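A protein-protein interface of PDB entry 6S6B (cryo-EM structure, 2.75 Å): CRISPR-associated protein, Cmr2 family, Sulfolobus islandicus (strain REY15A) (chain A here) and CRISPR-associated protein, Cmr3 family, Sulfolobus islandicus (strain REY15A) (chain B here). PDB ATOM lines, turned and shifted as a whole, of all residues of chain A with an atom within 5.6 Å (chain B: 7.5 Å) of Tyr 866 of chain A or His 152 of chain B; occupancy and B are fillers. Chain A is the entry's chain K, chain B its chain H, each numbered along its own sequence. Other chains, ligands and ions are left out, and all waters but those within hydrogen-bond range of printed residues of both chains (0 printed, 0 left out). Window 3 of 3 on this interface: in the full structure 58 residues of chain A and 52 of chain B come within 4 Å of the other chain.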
ATOM      1  N   THR A 558       3.667 -20.409 -26.102  1.00  0.00           N
ATOM      2  CA  THR A 558       2.879 -20.673 -24.907  1.00  0.00           C
ATOM      3  C   THR A 558       1.706 -21.598 -25.192  1.00  0.00           C
ATOM      4  O   THR A 558       1.153 -22.184 -24.258  1.00  0.00           O
ATOM      5  CB  THR A 558       2.375 -19.366 -24.304  1.00  0.00           C
ATOM      6  OG1 THR A 558       1.499 -18.720 -25.231  1.00  0.00           O
ATOM      7  CG2 THR A 558       3.530 -18.452 -23.994  1.00  0.00           C
ATOM      8  N   SER A 559       1.313 -21.741 -26.455  1.00  0.00           N
ATOM      9  CA  SER A 559       0.299 -22.728 -26.795  1.00  0.00           C
ATOM     10  C   SER A 559       0.894 -24.122 -26.913  1.00  0.00           C
ATOM     11  O   SER A 559       0.201 -25.110 -26.662  1.00  0.00           O
ATOM     12  CB  SER A 559      -0.401 -22.336 -28.094  1.00  0.00           C
ATOM     13  OG  SER A 559       0.541 -22.025 -29.102  1.00  0.00           O
ATOM     14  N   ALA A 562       1.335 -25.387 -23.288  1.00  0.00           N
ATOM     15  CA  ALA A 562       0.039 -25.739 -22.733  1.00  0.00           C
ATOM     16  C   ALA A 562      -0.554 -26.990 -23.364  1.00  0.00           C
ATOM     17  O   ALA A 562      -1.721 -27.300 -23.111  1.00  0.00           O
ATOM     18  CB  ALA A 562      -0.932 -24.570 -22.894  1.00  0.00           C
ATOM     19  N   GLU A 616      -3.167 -23.506 -32.236  1.00  0.00           N
ATOM     20  CA  GLU A 616      -4.222 -22.523 -32.421  1.00  0.00           C
ATOM     21  C   GLU A 616      -4.950 -22.674 -33.750  1.00  0.00           C
ATOM     22  O   GLU A 616      -5.825 -21.857 -34.053  1.00  0.00           O
ATOM     23  CB  GLU A 616      -3.645 -21.116 -32.302  1.00  0.00           C
ATOM     24  CG  GLU A 616      -3.143 -20.787 -30.913  1.00  0.00           C
ATOM     25  CD  GLU A 616      -2.604 -19.379 -30.813  1.00  0.00           C
ATOM     26  OE1 GLU A 616      -1.648 -19.055 -31.547  1.00  0.00           O
ATOM     27  OE2 GLU A 616      -3.138 -18.593 -30.005  1.00  0.00           O
ATOM     28  N   PHE A 620      -6.936 -25.552 -29.790  1.00  0.00           N
ATOM     29  CA  PHE A 620      -6.977 -24.183 -29.296  1.00  0.00           C
ATOM     30  C   PHE A 620      -7.512 -23.199 -30.327  1.00  0.00           C
ATOM     31  O   PHE A 620      -7.322 -21.990 -30.172  1.00  0.00           O
ATOM     32  CB  PHE A 620      -5.590 -23.742 -28.831  1.00  0.00           C
ATOM     33  CG  PHE A 620      -5.197 -24.295 -27.502  1.00  0.00           C
ATOM     34  CD1 PHE A 620      -6.154 -24.621 -26.567  1.00  0.00           C
ATOM     35  CD2 PHE A 620      -3.871 -24.485 -27.186  1.00  0.00           C
ATOM     36  CE1 PHE A 620      -5.798 -25.127 -25.348  1.00  0.00           C
ATOM     37  CE2 PHE A 620      -3.510 -24.989 -25.966  1.00  0.00           C
ATOM     38  CZ  PHE A 620      -4.475 -25.311 -25.047  1.00  0.00           C
ATOM     39  N   GLU A 622     -10.841 -21.883 -33.083  1.00  0.00           N
ATOM     40  CA  GLU A 622     -12.262 -21.569 -33.031  1.00  0.00           C
ATOM     41  C   GLU A 622     -13.062 -22.232 -34.137  1.00  0.00           C
ATOM     42  O   GLU A 622     -14.181 -22.690 -33.896  1.00  0.00           O
ATOM     43  CB  GLU A 622     -12.453 -20.052 -33.082  1.00  0.00           C
ATOM     44  CG  GLU A 622     -11.975 -19.368 -31.812  1.00  0.00           C
ATOM     45  CD  GLU A 622     -10.461 -19.250 -31.741  1.00  0.00           C
ATOM     46  OE1 GLU A 622      -9.786 -19.584 -32.738  1.00  0.00           O
ATOM     47  OE2 GLU A 622      -9.946 -18.853 -30.676  1.00  0.00           O
ATOM     48  N   ARG A 625     -12.378 -26.061 -32.787  1.00  0.00           N
ATOM     49  CA  ARG A 625     -12.379 -26.430 -31.375  1.00  0.00           C
ATOM     50  C   ARG A 625     -13.258 -27.647 -31.124  1.00  0.00           C
ATOM     51  O   ARG A 625     -12.796 -28.661 -30.595  1.00  0.00           O
ATOM     52  CB  ARG A 625     -12.841 -25.251 -30.520  1.00  0.00           C
ATOM     53  CG  ARG A 625     -12.909 -25.574 -29.039  1.00  0.00           C
ATOM     54  CD  ARG A 625     -13.496 -24.430 -28.228  1.00  0.00           C
ATOM     55  NE  ARG A 625     -12.800 -23.168 -28.447  1.00  0.00           N
ATOM     56  CZ  ARG A 625     -11.598 -22.881 -27.957  1.00  0.00           C
ATOM     57  NH1 ARG A 625     -10.949 -23.771 -27.220  1.00  0.00           N
ATOM     58  NH2 ARG A 625     -11.044 -21.703 -28.204  1.00  0.00           N
ATOM     59  N   PRO A 642      -5.635 -24.330 -21.306  1.00  0.00           N
ATOM     60  CA  PRO A 642      -4.893 -23.242 -21.944  1.00  0.00           C
ATOM     61  C   PRO A 642      -3.809 -22.614 -21.083  1.00  0.00           C
ATOM     62  O   PRO A 642      -3.259 -21.586 -21.481  1.00  0.00           O
ATOM     63  CB  PRO A 642      -6.003 -22.225 -22.231  1.00  0.00           C
ATOM     64  CG  PRO A 642      -6.984 -22.462 -21.167  1.00  0.00           C
ATOM     65  CD  PRO A 642      -7.017 -23.938 -20.994  1.00  0.00           C
ATOM     66  N   TYR A 643      -3.477 -23.189 -19.937  1.00  0.00           N
ATOM     67  CA  TYR A 643      -2.598 -22.551 -18.973  1.00  0.00           C
ATOM     68  C   TYR A 643      -1.234 -23.213 -18.964  1.00  0.00           C
ATOM     69  O   TYR A 643      -1.126 -24.439 -19.005  1.00  0.00           O
ATOM     70  CB  TYR A 643      -3.200 -22.602 -17.572  1.00  0.00           C
ATOM     71  CG  TYR A 643      -4.413 -21.730 -17.423  1.00  0.00           C
ATOM     72  CD1 TYR A 643      -5.672 -22.207 -17.727  1.00  0.00           C
ATOM     73  CD2 TYR A 643      -4.296 -20.425 -16.993  1.00  0.00           C
ATOM     74  CE1 TYR A 643      -6.778 -21.412 -17.601  1.00  0.00           C
ATOM     75  CE2 TYR A 643      -5.395 -19.621 -16.865  1.00  0.00           C
ATOM     76  CZ  TYR A 643      -6.634 -20.119 -17.170  1.00  0.00           C
ATOM     77  OH  TYR A 643      -7.737 -19.312 -17.040  1.00  0.00           O
ATOM     78  N   TYR A 644      -0.197 -22.393 -18.918  1.00  0.00           N
ATOM     79  CA  TYR A 644       1.159 -22.833 -18.658  1.00  0.00           C
ATOM     80  C   TYR A 644       1.640 -22.150 -17.386  1.00  0.00           C
ATOM     81  O   TYR A 644       0.913 -21.384 -16.757  1.00  0.00           O
ATOM     82  CB  TYR A 644       2.079 -22.524 -19.840  1.00  0.00           C
ATOM     83  CG  TYR A 644       2.285 -21.054 -20.073  1.00  0.00           C
ATOM     84  CD1 TYR A 644       1.298 -20.283 -20.650  1.00  0.00           C
ATOM     85  CD2 TYR A 644       3.464 -20.435 -19.708  1.00  0.00           C
ATOM     86  CE1 TYR A 644       1.479 -18.948 -20.855  1.00  0.00           C
ATOM     87  CE2 TYR A 644       3.651 -19.100 -19.911  1.00  0.00           C
ATOM     88  CZ  TYR A 644       2.656 -18.361 -20.484  1.00  0.00           C
ATOM     89  OH  TYR A 644       2.834 -17.019 -20.693  1.00  0.00           O
ATOM     90  N   ALA A 864      -0.400 -18.671 -16.202  1.00  0.00           N
ATOM     91  CA  ALA A 864      -0.938 -17.715 -17.152  1.00  0.00           C
ATOM     92  C   ALA A 864      -1.599 -18.432 -18.315  1.00  0.00           C
ATOM     93  O   ALA A 864      -1.138 -19.487 -18.751  1.00  0.00           O
ATOM     94  CB  ALA A 864       0.158 -16.796 -17.674  1.00  0.00           C
ATOM     95  N   HIS A 865      -2.690 -17.853 -18.800  1.00  0.00           N
ATOM     96  CA  HIS A 865      -3.292 -18.300 -20.043  1.00  0.00           C
ATOM     97  C   HIS A 865      -2.290 -18.143 -21.179  1.00  0.00           C
ATOM     98  O   HIS A 865      -1.488 -17.210 -21.189  1.00  0.00           O
ATOM     99  CB  HIS A 865      -4.545 -17.478 -20.317  1.00  0.00           C
ATOM    100  CG  HIS A 865      -5.520 -18.133 -21.239  1.00  0.00           C
ATOM    101  ND1 HIS A 865      -5.383 -18.102 -22.607  1.00  0.00           N
ATOM    102  CD2 HIS A 865      -6.662 -18.809 -20.989  1.00  0.00           C
ATOM    103  CE1 HIS A 865      -6.395 -18.742 -23.162  1.00  0.00           C
ATOM    104  NE2 HIS A 865      -7.185 -19.184 -22.202  1.00  0.00           N
ATOM    105  N   TYR A 866      -2.325 -19.067 -22.138  1.00  0.00           N
ATOM    106  CA  TYR A 866      -1.404 -18.966 -23.263  1.00  0.00           C
ATOM    107  C   TYR A 866      -1.628 -17.697 -24.065  1.00  0.00           C
ATOM    108  O   TYR A 866      -0.732 -17.275 -24.800  1.00  0.00           O
ATOM    109  CB  TYR A 866      -1.530 -20.188 -24.179  1.00  0.00           C
ATOM    110  CG  TYR A 866      -2.779 -20.199 -25.028  1.00  0.00           C
ATOM    111  CD1 TYR A 866      -2.820 -19.553 -26.251  1.00  0.00           C
ATOM    112  CD2 TYR A 866      -3.915 -20.858 -24.604  1.00  0.00           C
ATOM    113  CE1 TYR A 866      -3.957 -19.556 -27.015  1.00  0.00           C
ATOM    114  CE2 TYR A 866      -5.052 -20.869 -25.363  1.00  0.00           C
ATOM    115  CZ  TYR A 866      -5.069 -20.216 -26.567  1.00  0.00           C
ATOM    116  OH  TYR A 866      -6.211 -20.227 -27.329  1.00  0.00           O
ATOM    117  N   ALA A 867      -2.799 -17.083 -23.944  1.00  0.00           N
ATOM    118  CA  ALA A 867      -3.143 -15.891 -24.695  1.00  0.00           C
ATOM    119  C   ALA A 867      -2.889 -14.608 -23.922  1.00  0.00           C
ATOM    120  O   ALA A 867      -3.175 -13.526 -24.438  1.00  0.00           O
ATOM    121  CB  ALA A 867      -4.608 -15.948 -25.127  1.00  0.00           C
ATOM    122  N   ASP A 868      -2.374 -14.699 -22.705  1.00  0.00           N
ATOM    123  CA  ASP A 868      -2.109 -13.498 -21.933  1.00  0.00           C
ATOM    124  C   ASP A 868      -0.905 -12.766 -22.516  1.00  0.00           C
ATOM    125  O   ASP A 868       0.044 -13.403 -22.979  1.00  0.00           O
ATOM    126  CB  ASP A 868      -1.849 -13.845 -20.472  1.00  0.00           C
ATOM    127  CG  ASP A 868      -3.124 -14.062 -19.689  1.00  0.00           C
ATOM    128  OD1 ASP A 868      -4.177 -13.547 -20.112  1.00  0.00           O
ATOM    129  OD2 ASP A 868      -3.074 -14.746 -18.648  1.00  0.00           O
ATOM    130  N   PRO B  22      -8.234  -4.814 -29.163  1.00  0.00           N
ATOM    131  CA  PRO B  22      -8.012  -6.145 -29.736  1.00  0.00           C
ATOM    132  C   PRO B  22      -7.528  -6.085 -31.175  1.00  0.00           C
ATOM    133  O   PRO B  22      -8.289  -5.739 -32.083  1.00  0.00           O
ATOM    134  CB  PRO B  22      -9.389  -6.804 -29.629  1.00  0.00           C
ATOM    135  CG  PRO B  22     -10.347  -5.679 -29.638  1.00  0.00           C
ATOM    136  CD  PRO B  22      -9.665  -4.489 -29.042  1.00  0.00           C
ATOM    137  N   ILE B  24      -4.436  -8.509 -32.355  1.00  0.00           N
ATOM    138  CA  ILE B  24      -4.014  -9.869 -32.661  1.00  0.00           C
ATOM    139  C   ILE B  24      -5.123 -10.833 -32.263  1.00  0.00           C
ATOM    140  O   ILE B  24      -5.853 -10.609 -31.295  1.00  0.00           O
ATOM    141  CB  ILE B  24      -2.684 -10.192 -31.952  1.00  0.00           C
ATOM    142  CG1 ILE B  24      -1.622  -9.162 -32.335  1.00  0.00           C
ATOM    143  CG2 ILE B  24      -2.200 -11.578 -32.316  1.00  0.00           C
ATOM    144  CD1 ILE B  24      -1.417  -8.074 -31.317  1.00  0.00           C
ATOM    145  N   THR B  25      -5.258 -11.918 -33.023  1.00  0.00           N
ATOM    146  CA  THR B  25      -6.401 -12.806 -32.845  1.00  0.00           C
ATOM    147  C   THR B  25      -6.250 -13.676 -31.603  1.00  0.00           C
ATOM    148  O   THR B  25      -7.098 -13.648 -30.705  1.00  0.00           O
ATOM    149  CB  THR B  25      -6.584 -13.680 -34.084  1.00  0.00           C
ATOM    150  OG1 THR B  25      -5.511 -14.625 -34.159  1.00  0.00           O
ATOM    151  CG2 THR B  25      -6.582 -12.822 -35.334  1.00  0.00           C
ATOM    152  N   GLY B  26      -5.184 -14.462 -31.538  1.00  0.00           N
ATOM    153  CA  GLY B  26      -5.032 -15.392 -30.439  1.00  0.00           C
ATOM    154  C   GLY B  26      -4.274 -14.814 -29.267  1.00  0.00           C
ATOM    155  O   GLY B  26      -3.276 -15.392 -28.829  1.00  0.00           O
ATOM    156  N   SER B  27      -4.735 -13.682 -28.744  1.00  0.00           N
ATOM    157  CA  SER B  27      -4.009 -13.010 -27.679  1.00  0.00           C
ATOM    158  C   SER B  27      -4.922 -12.013 -26.987  1.00  0.00           C
ATOM    159  O   SER B  27      -5.734 -11.355 -27.636  1.00  0.00           O
ATOM    160  CB  SER B  27      -2.766 -12.299 -28.223  1.00  0.00           C
ATOM    161  OG  SER B  27      -2.339 -11.277 -27.345  1.00  0.00           O
ATOM    162  N   HIS B  28      -4.778 -11.914 -25.671  1.00  0.00           N
ATOM    163  CA  HIS B  28      -5.499 -10.928 -24.889  1.00  0.00           C
ATOM    164  C   HIS B  28      -4.783  -9.586 -24.945  1.00  0.00           C
ATOM    165  O   HIS B  28      -3.639  -9.480 -25.386  1.00  0.00           O
ATOM    166  CB  HIS B  28      -5.626 -11.382 -23.440  1.00  0.00           C
ATOM    167  CG  HIS B  28      -6.324 -12.692 -23.271  1.00  0.00           C
ATOM    168  ND1 HIS B  28      -7.343 -13.104 -24.098  1.00  0.00           N
ATOM    169  CD2 HIS B  28      -6.154 -13.679 -22.363  1.00  0.00           C
ATOM    170  CE1 HIS B  28      -7.767 -14.293 -23.710  1.00  0.00           C
ATOM    171  NE2 HIS B  28      -7.063 -14.664 -22.658  1.00  0.00           N
ATOM    172  N   THR B  29      -5.472  -8.549 -24.489  1.00  0.00           N
ATOM    173  CA  THR B  29      -4.871  -7.238 -24.313  1.00  0.00           C
ATOM    174  C   THR B  29      -4.811  -6.897 -22.833  1.00  0.00           C
ATOM    175  O   THR B  29      -5.553  -7.441 -22.018  1.00  0.00           O
ATOM    176  CB  THR B  29      -5.645  -6.156 -25.066  1.00  0.00           C
ATOM    177  OG1 THR B  29      -7.048  -6.358 -24.894  1.00  0.00           O
ATOM    178  CG2 THR B  29      -5.316  -6.209 -26.536  1.00  0.00           C
ATOM    179  N   ILE B 140     -14.475  -7.867 -21.195  1.00  0.00           N
ATOM    180  CA  ILE B 140     -14.835  -8.909 -22.142  1.00  0.00           C
ATOM    181  C   ILE B 140     -15.811  -8.334 -23.148  1.00  0.00           C
ATOM    182  O   ILE B 140     -16.635  -7.482 -22.815  1.00  0.00           O
ATOM    183  CB  ILE B 140     -15.409 -10.142 -21.399  1.00  0.00           C
ATOM    184  CG1 ILE B 140     -14.318 -11.187 -21.212  1.00  0.00           C
ATOM    185  CG2 ILE B 140     -16.648 -10.701 -22.070  1.00  0.00           C
ATOM    186  CD1 ILE B 140     -14.752 -12.342 -20.417  1.00  0.00           C
ATOM    187  N   SER B 141     -15.703  -8.789 -24.389  1.00  0.00           N
ATOM    188  CA  SER B 141     -16.636  -8.433 -25.445  1.00  0.00           C
ATOM    189  C   SER B 141     -17.440  -9.666 -25.825  1.00  0.00           C
ATOM    190  O   SER B 141     -16.870 -10.725 -26.094  1.00  0.00           O
ATOM    191  CB  SER B 141     -15.899  -7.875 -26.660  1.00  0.00           C
ATOM    192  OG  SER B 141     -16.812  -7.511 -27.674  1.00  0.00           O
ATOM    193  N   VAL B 149     -18.280 -15.156 -24.847  1.00  0.00           N
ATOM    194  CA  VAL B 149     -17.170 -14.261 -25.142  1.00  0.00           C
ATOM    195  C   VAL B 149     -16.694 -14.510 -26.566  1.00  0.00           C
ATOM    196  O   VAL B 149     -16.773 -15.627 -27.086  1.00  0.00           O
ATOM    197  CB  VAL B 149     -16.030 -14.441 -24.119  1.00  0.00           C
ATOM    198  CG1 VAL B 149     -15.342 -15.761 -24.322  1.00  0.00           C
ATOM    199  CG2 VAL B 149     -15.036 -13.307 -24.219  1.00  0.00           C
ATOM    200  N   LYS B 150     -16.211 -13.457 -27.213  1.00  0.00           N
ATOM    201  CA  LYS B 150     -15.721 -13.560 -28.579  1.00  0.00           C
ATOM    202  C   LYS B 150     -14.375 -14.278 -28.586  1.00  0.00           C
ATOM    203  O   LYS B 150     -13.895 -14.780 -27.568  1.00  0.00           O
ATOM    204  CB  LYS B 150     -15.625 -12.182 -29.215  1.00  0.00           C
ATOM    205  CG  LYS B 150     -16.952 -11.626 -29.652  1.00  0.00           C
ATOM    206  CD  LYS B 150     -16.834 -10.194 -30.120  1.00  0.00           C
ATOM    207  CE  LYS B 150     -16.234 -10.121 -31.503  1.00  0.00           C
ATOM    208  NZ  LYS B 150     -16.501  -8.800 -32.134  1.00  0.00           N
ATOM    209  N   GLU B 151     -13.744 -14.332 -29.751  1.00  0.00           N
ATOM    210  CA  GLU B 151     -12.462 -15.006 -29.857  1.00  0.00           C
ATOM    211  C   GLU B 151     -11.381 -14.186 -29.171  1.00  0.00           C
ATOM    212  O   GLU B 151     -10.787 -13.294 -29.784  1.00  0.00           O
ATOM    213  CB  GLU B 151     -12.098 -15.244 -31.322  1.00  0.00           C
ATOM    214  CG  GLU B 151     -10.729 -15.859 -31.521  1.00  0.00           C
ATOM    215  CD  GLU B 151     -10.249 -15.769 -32.952  1.00  0.00           C
ATOM    216  OE1 GLU B 151     -11.003 -15.242 -33.796  1.00  0.00           O
ATOM    217  OE2 GLU B 151      -9.123 -16.229 -33.234  1.00  0.00           O
ATOM    218  N   HIS B 152     -11.132 -14.475 -27.895  1.00  0.00           N
ATOM    219  CA  HIS B 152     -10.042 -13.869 -27.140  1.00  0.00           C
ATOM    220  C   HIS B 152     -10.204 -12.362 -26.984  1.00  0.00           C
ATOM    221  O   HIS B 152      -9.216 -11.639 -26.857  1.00  0.00           O
ATOM    222  CB  HIS B 152      -8.690 -14.185 -27.778  1.00  0.00           C
ATOM    223  CG  HIS B 152      -8.324 -15.631 -27.726  1.00  0.00           C
ATOM    224  ND1 HIS B 152      -7.741 -16.288 -28.786  1.00  0.00           N
ATOM    225  CD2 HIS B 152      -8.454 -16.548 -26.739  1.00  0.00           C
ATOM    226  CE1 HIS B 152      -7.525 -17.548 -28.454  1.00  0.00           C
ATOM    227  NE2 HIS B 152      -7.950 -17.732 -27.217  1.00  0.00           N
ATOM    228  N   TYR B 153     -11.436 -11.864 -26.987  1.00  0.00           N
ATOM    229  CA  TYR B 153     -11.678 -10.446 -26.732  1.00  0.00           C
ATOM    230  C   TYR B 153     -11.784 -10.195 -25.230  1.00  0.00           C
ATOM    231  O   TYR B 153     -12.804  -9.766 -24.702  1.00  0.00           O
ATOM    232  CB  TYR B 153     -12.926  -9.975 -27.463  1.00  0.00           C
ATOM    233  CG  TYR B 153     -12.684  -9.637 -28.909  1.00  0.00           C
ATOM    234  CD1 TYR B 153     -11.943 -10.475 -29.721  1.00  0.00           C
ATOM    235  CD2 TYR B 153     -13.195  -8.478 -29.462  1.00  0.00           C
ATOM    236  CE1 TYR B 153     -11.722 -10.179 -31.034  1.00  0.00           C
ATOM    237  CE2 TYR B 153     -12.975  -8.171 -30.780  1.00  0.00           C
ATOM    238  CZ  TYR B 153     -12.238  -9.026 -31.559  1.00  0.00           C
ATOM    239  OH  TYR B 153     -12.015  -8.724 -32.879  1.00  0.00           O
ATOM    240  N   LEU B 154     -10.684 -10.480 -24.549  1.00  0.00           N
ATOM    241  CA  LEU B 154     -10.566 -10.314 -23.111  1.00  0.00           C
ATOM    242  C   LEU B 154      -9.404  -9.380 -22.826  1.00  0.00           C
ATOM    243  O   LEU B 154      -8.340  -9.499 -23.435  1.00  0.00           O
ATOM    244  CB  LEU B 154     -10.350 -11.663 -22.427  1.00  0.00           C
ATOM    245  CG  LEU B 154     -10.242 -11.716 -20.907  1.00  0.00           C
ATOM    246  CD1 LEU B 154     -11.003 -12.905 -20.393  1.00  0.00           C
ATOM    247  CD2 LEU B 154      -8.800 -11.803 -20.473  1.00  0.00           C
ATOM    248  N   TYR B 155      -9.609  -8.444 -21.907  1.00  0.00           N
ATOM    249  CA  TYR B 155      -8.583  -7.471 -21.583  1.00  0.00           C
ATOM    250  C   TYR B 155      -8.527  -7.246 -20.084  1.00  0.00           C
ATOM    251  O   TYR B 155      -9.560  -7.234 -19.411  1.00  0.00           O
ATOM    252  CB  TYR B 155      -8.829  -6.142 -22.290  1.00  0.00           C
ATOM    253  CG  TYR B 155     -10.114  -5.467 -21.911  1.00  0.00           C
ATOM    254  CD1 TYR B 155     -11.286  -5.745 -22.585  1.00  0.00           C
ATOM    255  CD2 TYR B 155     -10.156  -4.544 -20.885  1.00  0.00           C
ATOM    256  CE1 TYR B 155     -12.461  -5.125 -22.250  1.00  0.00           C
ATOM    257  CE2 TYR B 155     -11.325  -3.920 -20.539  1.00  0.00           C
ATOM    258  CZ  TYR B 155     -12.475  -4.212 -21.226  1.00  0.00           C
ATOM    259  OH  TYR B 155     -13.650  -3.593 -20.882  1.00  0.00           O
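A ring nitrogen (NE2) of His 152 of chain B lies within hydrogen-bond range of the side-chain hydroxyl (OH) of Tyr 866 of chain A (3.0 Å). OE2 of Glu 151 of chain B lies close to OE1 of Glu 622 of chain A (3.5 Å). The backbone carbonyl oxygen (O) of Ala 867 of chain A sits at hydrogen-bond distance from the backbone NH (N) of His 28 of chain B (2.6 Å). OE2 of Glu 616 of chain A sits close to O of Gly 26 of chain B (3.4 Å).
N of His 865 of chain A lies within hydrogen-bond range of OD2 of Asp 868 of chain A (3.1 Å). O of Pro 642 of chain A is in hydrogen-bond range of N of Tyr 866 of chain A (2.8 Å). The backbone carbonyl oxygen (O) of Tyr 866 of chain A sits at hydrogen-bond distance from the side-chain hydroxyl (OG1) of Thr 558 of chain A (2.7 Å). ND1 of His 152 of chain B lies within hydrogen-bond range of O of Thr 25 of chain B, at 3.3 Å. OE2 of Glu 622 of chain A lies within salt-bridge range of NH2 of Arg 625 of chain A. A ring nitrogen (ND1) of His 865 of chain A lies close to the backbone NH of Ala 867 of chain A.
CE1 of His 152 of chain B touches OE2 of Glu 622 of chain A (3.5 Å). ND1 of His 865 of chain A touches NE2 of His 28 of chain B, 3.8 Å away. Ala 867 of chain A touches Gly 26 of chain B. Ala 867 of chain A touches Ser 27 of chain B (O to CA, 3.4 Å). Asp 868 of chain A touches His 28 of chain B.
Of the printed residues of chain B, Glu 616 of chain A touches Gly 26 (3.4 Å). Printed residues of chain B within 4 Å of Glu 622 of chain A: Glu 151 (3.2 Å) and His 152 (3.5 Å). Pro 642 of chain A touches none of the printed residues of chain B. Of the printed residues of chain B, His 865 of chain A touches His 28 (3.8 Å). Tyr 866 of chain A touches just one residue of chain B: His 152. Printed residues of chain B within 4 Å of Ala 867 of chain A: Gly 26 (3.97 Å), Ser 27 (3.4 Å) and His 28 (2.6 Å). Printed residues of chain A within 4 Å of His 28 of chain B: His 865 (3.8 Å), Ala 867 (2.6 Å) and Asp 868 (3.0 Å). His 152 of chain B touches two residues of chain A. The nearest printed residue of chain A that does not touch Gly 26 of chain B is Tyr 866 of chain A (4.6 Å).
Printed residues of chain A that touch a printed residue of chain B: Glu 616, Glu 622, His 865, Tyr 866, Ala 867 and Asp 868. Hydrophobic or aromatic side chains of chain A that line the printed part of chain B: His 865, Tyr 866 and Ala 867. Hydrophobic or aromatic side chains of chain B within 4 Å of the printed part of chain A: His 28 and His 152. Among the printed residues, no Asp or Glu carboxylate lies within 4 Å of a Lys or Arg side-chain nitrogen of the other chain.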
